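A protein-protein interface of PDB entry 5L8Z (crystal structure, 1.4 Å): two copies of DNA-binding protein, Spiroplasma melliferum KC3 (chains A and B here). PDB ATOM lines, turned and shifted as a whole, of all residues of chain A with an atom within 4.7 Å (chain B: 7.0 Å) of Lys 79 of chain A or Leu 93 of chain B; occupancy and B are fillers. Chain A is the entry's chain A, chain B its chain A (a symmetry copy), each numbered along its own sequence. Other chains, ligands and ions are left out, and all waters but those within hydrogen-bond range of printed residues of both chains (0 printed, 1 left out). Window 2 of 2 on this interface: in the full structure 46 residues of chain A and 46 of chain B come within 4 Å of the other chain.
No position is printed for both chains.
Of the 11 pairs that touch across the chains among the printed residues, none has its exchanged pair printed and touching as well.
The backbone carbonyl oxygen of Thr 57 of chain A sits at hydrogen-bond distance from the backbone NH of Ser 80 of chain A (2.8 Å).
NZ of Lys 79 of chain A lies within salt-bridge range of OE2 of Glu 58 of chain A (3.2 Å).
The backbone carbonyl oxygen of Lys 90 of chain B lies within hydrogen-bond range of the side-chain amide nitrogen of Asn 94 of chain B.
Of chain B, only Leu 93 and Asn 94 come within 4 Å of Lys 79 of chain A.
Leu 93 of chain B touches six residues of chain A.
Printed residues of chain B within 4 Å of Ala 81 of chain A: Leu 93 (3.97 Å).
Printed residues of chain A within 4 Å of Asp 92 of chain B: Val 41.
The nearest printed residue of chain A that does not touch Leu 93 of chain B is Thr 57 of chain A (6.1 Å).
CD2 of Leu 93 of chain B touches O of Leu 40 of chain A, at 3.7 Å.
CG2 of Val 41 of chain A touches CB of Asp 92 of chain B (3.7 Å).
Val 41 of chain A touches Leu 93 of chain B.
CG2 of Val 56 of chain A touches CD2 of Leu 93 of chain B, at 3.9 Å.
Asn 94 of chain B touches Ser 78 of chain A.
Lys 79 of chain A touches Leu 93 of chain B (CD to O, 3.5 Å).
Ser 80 of chain A touches Ala 85 of chain B (OG to CB, 3.9 Å).
Lys 90 of chain B touches Ser 80 of chain A.
Ser 80 of chain A touches Leu 93 of chain B.
Leu 93 of chain B touches Ala 81 of chain A (CD1 to N, 3.97 Å).
Of the 10 printed residues of chain A, 7 touch a printed residue of chain B.
Hydrophobic or aromatic side chains of chain A within 4 Å of the printed part of chain B: Val 41, Val 56 and Ala 81.
Of the 10 printed residues of chain B, 5 touch a printed residue of chain A.
Printed residues of chain B that touch a printed residue of chain A: Ala 85, Lys 90, Asp 92, Leu 93 and Asn 94.
Hydrophobic or aromatic side chains of chain B that line the printed part of chain A: Ala 85 and Leu 93.
The backbone NH (N) of Lys 79 of chain A lies within hydrogen-bond range of the side-chain amide oxygen (OD1) of Asn 94 of chain B, at 2.8 Å.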
ATOM      1  N   LEU A  40      -5.849  21.185  -0.821  1.00  0.00           N
ATOM      2  CA  LEU A  40      -5.248  21.106  -2.141  1.00  0.00           C
ATOM      3  C   LEU A  40      -4.107  20.159  -2.166  1.00  0.00           C
ATOM      4  O   LEU A  40      -3.960  19.391  -3.114  1.00  0.00           O
ATOM      5  CB  LEU A  40      -4.777  22.514  -2.492  1.00  0.00           C
ATOM      6  CG  LEU A  40      -5.916  23.502  -2.706  1.00  0.00           C
ATOM      7  CD1 LEU A  40      -5.351  24.882  -2.696  1.00  0.00           C
ATOM      8  CD2 LEU A  40      -6.709  23.205  -3.997  1.00  0.00           C
ATOM      9  N   VAL A  41      -3.310  20.152  -1.108  1.00  0.00           N
ATOM     10  CA  VAL A  41      -2.178  19.226  -1.036  1.00  0.00           C
ATOM     11  C   VAL A  41      -2.680  17.808  -1.047  1.00  0.00           C
ATOM     12  O   VAL A  41      -2.033  16.908  -1.594  1.00  0.00           O
ATOM     13  CB  VAL A  41      -1.323  19.559   0.210  1.00  0.00           C
ATOM     14  CG1 VAL A  41      -0.306  18.417   0.495  1.00  0.00           C
ATOM     15  CG2 VAL A  41      -0.592  20.876   0.014  1.00  0.00           C
ATOM     16  N   VAL A  56      -5.900  21.958  -7.776  1.00  0.00           N
ATOM     17  CA  VAL A  56      -4.523  21.705  -8.111  1.00  0.00           C
ATOM     18  C   VAL A  56      -4.474  21.423  -9.584  1.00  0.00           C
ATOM     19  O   VAL A  56      -5.273  20.727 -10.122  1.00  0.00           O
ATOM     20  CB  VAL A  56      -4.011  20.482  -7.365  1.00  0.00           C
ATOM     21  CG1 VAL A  56      -2.531  20.270  -7.770  1.00  0.00           C
ATOM     22  CG2 VAL A  56      -4.096  20.745  -5.879  1.00  0.00           C
ATOM     23  N   THR A  57      -3.447  22.029 -10.174  1.00  0.00           N
ATOM     24  CA  THR A  57      -3.196  21.922 -11.575  1.00  0.00           C
ATOM     25  C   THR A  57      -1.805  21.332 -11.665  1.00  0.00           C
ATOM     26  O   THR A  57      -1.000  21.362 -10.686  1.00  0.00           O
ATOM     27  CB  THR A  57      -3.064  23.315 -12.237  1.00  0.00           C
ATOM     28  OG1 THR A  57      -2.092  24.122 -11.521  1.00  0.00           O
ATOM     29  CG2 THR A  57      -4.406  23.971 -12.186  1.00  0.00           C
ATOM     30  N   GLU A  58      -1.566  20.686 -12.797  1.00  0.00           N
ATOM     31  CA  GLU A  58      -0.195  20.193 -13.030  1.00  0.00           C
ATOM     32  C   GLU A  58       0.197  20.620 -14.424  1.00  0.00           C
ATOM     33  O   GLU A  58      -0.462  20.285 -15.363  1.00  0.00           O
ATOM     34  CB  GLU A  58      -0.150  18.662 -12.864  1.00  0.00           C
ATOM     35  CG  GLU A  58       1.256  18.104 -13.132  1.00  0.00           C
ATOM     36  CD  GLU A  58       1.432  16.673 -12.646  1.00  0.00           C
ATOM     37  OE1 GLU A  58       0.756  15.816 -13.156  1.00  0.00           O
ATOM     38  OE2 GLU A  58       2.295  16.449 -11.782  1.00  0.00           O
ATOM     39  N   ALA A  77       7.101  17.876 -14.979  1.00  0.00           N
ATOM     40  CA  ALA A  77       5.776  18.285 -14.526  1.00  0.00           C
ATOM     41  C   ALA A  77       5.935  19.110 -13.255  1.00  0.00           C
ATOM     42  O   ALA A  77       6.906  18.978 -12.492  1.00  0.00           O
ATOM     43  CB  ALA A  77       4.889  17.060 -14.298  1.00  0.00           C
ATOM     44  N   SER A  78       4.990  20.019 -12.991  1.00  0.00           N
ATOM     45  CA  SER A  78       5.002  20.706 -11.711  1.00  0.00           C
ATOM     46  C   SER A  78       3.546  21.027 -11.422  1.00  0.00           C
ATOM     47  O   SER A  78       2.704  21.072 -12.370  1.00  0.00           O
ATOM     48  CB  SER A  78       5.857  21.951 -11.722  1.00  0.00           C
ATOM     49  OG  SER A  78       5.498  22.786 -12.768  1.00  0.00           O
ATOM     50  N   LYS A  79       3.251  21.146 -10.140  1.00  0.00           N
ATOM     51  CA  LYS A  79       1.907  21.388  -9.699  1.00  0.00           C
ATOM     52  C   LYS A  79       1.787  22.829  -9.258  1.00  0.00           C
ATOM     53  O   LYS A  79       2.716  23.482  -8.767  1.00  0.00           O
ATOM     54  CB  LYS A  79       1.560  20.485  -8.555  1.00  0.00           C
ATOM     55  CG  LYS A  79       1.546  19.053  -8.981  1.00  0.00           C
ATOM     56  CD  LYS A  79       0.922  18.145  -7.926  1.00  0.00           C
ATOM     57  CE  LYS A  79       1.041  16.671  -8.352  1.00  0.00           C
ATOM     58  NZ  LYS A  79       0.083  16.267  -9.431  1.00  0.00           N
ATOM     59  N   SER A  80       0.575  23.307  -9.431  1.00  0.00           N
ATOM     60  CA  SER A  80       0.258  24.631  -8.875  1.00  0.00           C
ATOM     61  C   SER A  80      -1.191  24.532  -8.438  1.00  0.00           C
ATOM     62  O   SER A  80      -1.697  23.446  -8.262  1.00  0.00           O
ATOM     63  CB  SER A  80       0.533  25.715  -9.858  1.00  0.00           C
ATOM     64  OG  SER A  80       0.384  26.967  -9.189  1.00  0.00           O
ATOM     65  N   ALA A  81      -1.783  25.649  -8.099  1.00  0.00           N
ATOM     66  CA  ALA A  81      -3.185  25.665  -7.736  1.00  0.00           C
ATOM     67  C   ALA A  81      -3.808  26.805  -8.528  1.00  0.00           C
ATOM     68  O   ALA A  81      -3.194  27.854  -8.741  1.00  0.00           O
ATOM     69  CB  ALA A  81      -3.286  25.937  -6.229  1.00  0.00           C
ATOM     70  N   ALA B  85      -0.870  31.525  -6.838  1.00  0.00           N
ATOM     71  CA  ALA B  85      -0.501  30.761  -5.705  1.00  0.00           C
ATOM     72  C   ALA B  85       0.841  31.251  -5.181  1.00  0.00           C
ATOM     73  O   ALA B  85       1.752  31.580  -6.001  1.00  0.00           O
ATOM     74  CB  ALA B  85      -0.405  29.288  -6.136  1.00  0.00           C
ATOM     75  N   LYS B  87       4.453  31.117  -2.984  1.00  0.00           N
ATOM     76  CA  LYS B  87       5.606  30.194  -3.016  1.00  0.00           C
ATOM     77  C   LYS B  87       5.372  29.045  -2.082  1.00  0.00           C
ATOM     78  O   LYS B  87       5.687  27.913  -2.433  1.00  0.00           O
ATOM     79  CB  LYS B  87       6.914  30.928  -2.666  1.00  0.00           C
ATOM     80  N   GLN B  88       4.842  29.273  -0.902  1.00  0.00           N
ATOM     81  CA  GLN B  88       4.712  28.199   0.056  1.00  0.00           C
ATOM     82  C   GLN B  88       3.682  27.152  -0.455  1.00  0.00           C
ATOM     83  O   GLN B  88       3.904  25.956  -0.316  1.00  0.00           O
ATOM     84  CB  GLN B  88       4.358  28.643   1.512  1.00  0.00           C
ATOM     85  CG  GLN B  88       5.270  29.725   2.123  1.00  0.00           C
ATOM     86  CD  GLN B  88       4.897  31.167   1.762  1.00  0.00           C
ATOM     87  OE1 GLN B  88       4.371  31.482   0.687  1.00  0.00           O
ATOM     88  NE2 GLN B  88       5.174  32.069   2.696  1.00  0.00           N
ATOM     89  N   LEU B  89       2.584  27.641  -1.022  1.00  0.00           N
ATOM     90  CA  LEU B  89       1.632  26.713  -1.562  1.00  0.00           C
ATOM     91  C   LEU B  89       2.242  25.916  -2.708  1.00  0.00           C
ATOM     92  O   LEU B  89       2.079  24.705  -2.778  1.00  0.00           O
ATOM     93  CB  LEU B  89       0.422  27.498  -2.022  1.00  0.00           C
ATOM     94  CG  LEU B  89      -0.671  26.651  -2.685  1.00  0.00           C
ATOM     95  CD1 LEU B  89      -1.089  25.471  -1.771  1.00  0.00           C
ATOM     96  CD2 LEU B  89      -1.799  27.674  -2.882  1.00  0.00           C
ATOM     97  N   LYS B  90       2.989  26.592  -3.560  1.00  0.00           N
ATOM     98  CA  LYS B  90       3.647  25.884  -4.637  1.00  0.00           C
ATOM     99  C   LYS B  90       4.626  24.874  -4.122  1.00  0.00           C
ATOM    100  O   LYS B  90       4.593  23.709  -4.535  1.00  0.00           O
ATOM    101  CB  LYS B  90       4.309  26.828  -5.558  1.00  0.00           C
ATOM    102  CG  LYS B  90       3.284  27.394  -6.505  1.00  0.00           C
ATOM    103  CD  LYS B  90       4.036  28.374  -7.332  1.00  0.00           C
ATOM    104  CE  LYS B  90       3.243  28.802  -8.533  1.00  0.00           C
ATOM    105  NZ  LYS B  90       4.021  30.008  -8.922  1.00  0.00           N
ATOM    106  N   THR B  91       5.375  25.246  -3.074  1.00  0.00           N
ATOM    107  CA  THR B  91       6.288  24.280  -2.486  1.00  0.00           C
ATOM    108  C   THR B  91       5.498  23.093  -1.964  1.00  0.00           C
ATOM    109  O   THR B  91       5.866  21.930  -2.243  1.00  0.00           O
ATOM    110  CB  THR B  91       7.019  24.981  -1.349  1.00  0.00           C
ATOM    111  OG1 THR B  91       7.869  25.965  -1.913  1.00  0.00           O
ATOM    112  CG2 THR B  91       7.843  23.990  -0.496  1.00  0.00           C
ATOM    113  N   ASP B  92       4.432  23.345  -1.213  1.00  0.00           N
ATOM    114  CA  ASP B  92       3.677  22.256  -0.556  1.00  0.00           C
ATOM    115  C   ASP B  92       3.083  21.325  -1.612  1.00  0.00           C
ATOM    116  O   ASP B  92       3.010  20.139  -1.395  1.00  0.00           O
ATOM    117  CB  ASP B  92       2.544  22.805   0.270  1.00  0.00           C
ATOM    118  CG  ASP B  92       3.025  23.526   1.563  1.00  0.00           C
ATOM    119  OD1 ASP B  92       4.204  23.409   1.884  1.00  0.00           O
ATOM    120  OD2 ASP B  92       2.207  24.242   2.114  1.00  0.00           O
ATOM    121  N   LEU B  93       2.713  21.860  -2.768  1.00  0.00           N
ATOM    122  CA  LEU B  93       2.109  21.025  -3.776  1.00  0.00           C
ATOM    123  C   LEU B  93       3.111  20.221  -4.531  1.00  0.00           C
ATOM    124  O   LEU B  93       2.716  19.311  -5.214  1.00  0.00           O
ATOM    125  CB  LEU B  93       1.370  21.877  -4.803  1.00  0.00           C
ATOM    126  CG  LEU B  93       0.163  22.477  -4.133  1.00  0.00           C
ATOM    127  CD1 LEU B  93      -0.337  23.536  -5.069  1.00  0.00           C
ATOM    128  CD2 LEU B  93      -0.902  21.433  -3.841  1.00  0.00           C
ATOM    129  N   ASN B  94       4.372  20.587  -4.450  1.00  0.00           N
ATOM    130  CA  ASN B  94       5.398  19.895  -5.191  1.00  0.00           C
ATOM    131  C   ASN B  94       6.315  19.003  -4.351  1.00  0.00           C
ATOM    132  O   ASN B  94       7.304  18.510  -4.833  1.00  0.00           O
ATOM    133  CB  ASN B  94       6.139  20.890  -6.027  1.00  0.00           C
ATOM    134  CG  ASN B  94       5.299  21.338  -7.166  1.00  0.00           C
ATOM    135  OD1 ASN B  94       5.136  20.637  -8.146  1.00  0.00           O
ATOM    136  ND2 ASN B  94       4.717  22.538  -7.022  1.00  0.00           N
ATOM    137  N   ASN B  95       5.882  18.760  -3.130  1.00  0.00           N
ATOM    138  CA  ASN B  95       6.641  17.936  -2.165  1.00  0.00           C
ATOM    139  C   ASN B  95       6.339  16.444  -2.268  1.00  0.00           C
ATOM    140  O   ASN B  95       5.179  16.044  -2.395  1.00  0.00           O
ATOM    141  CB  ASN B  95       6.383  18.427  -0.722  1.00  0.00           C
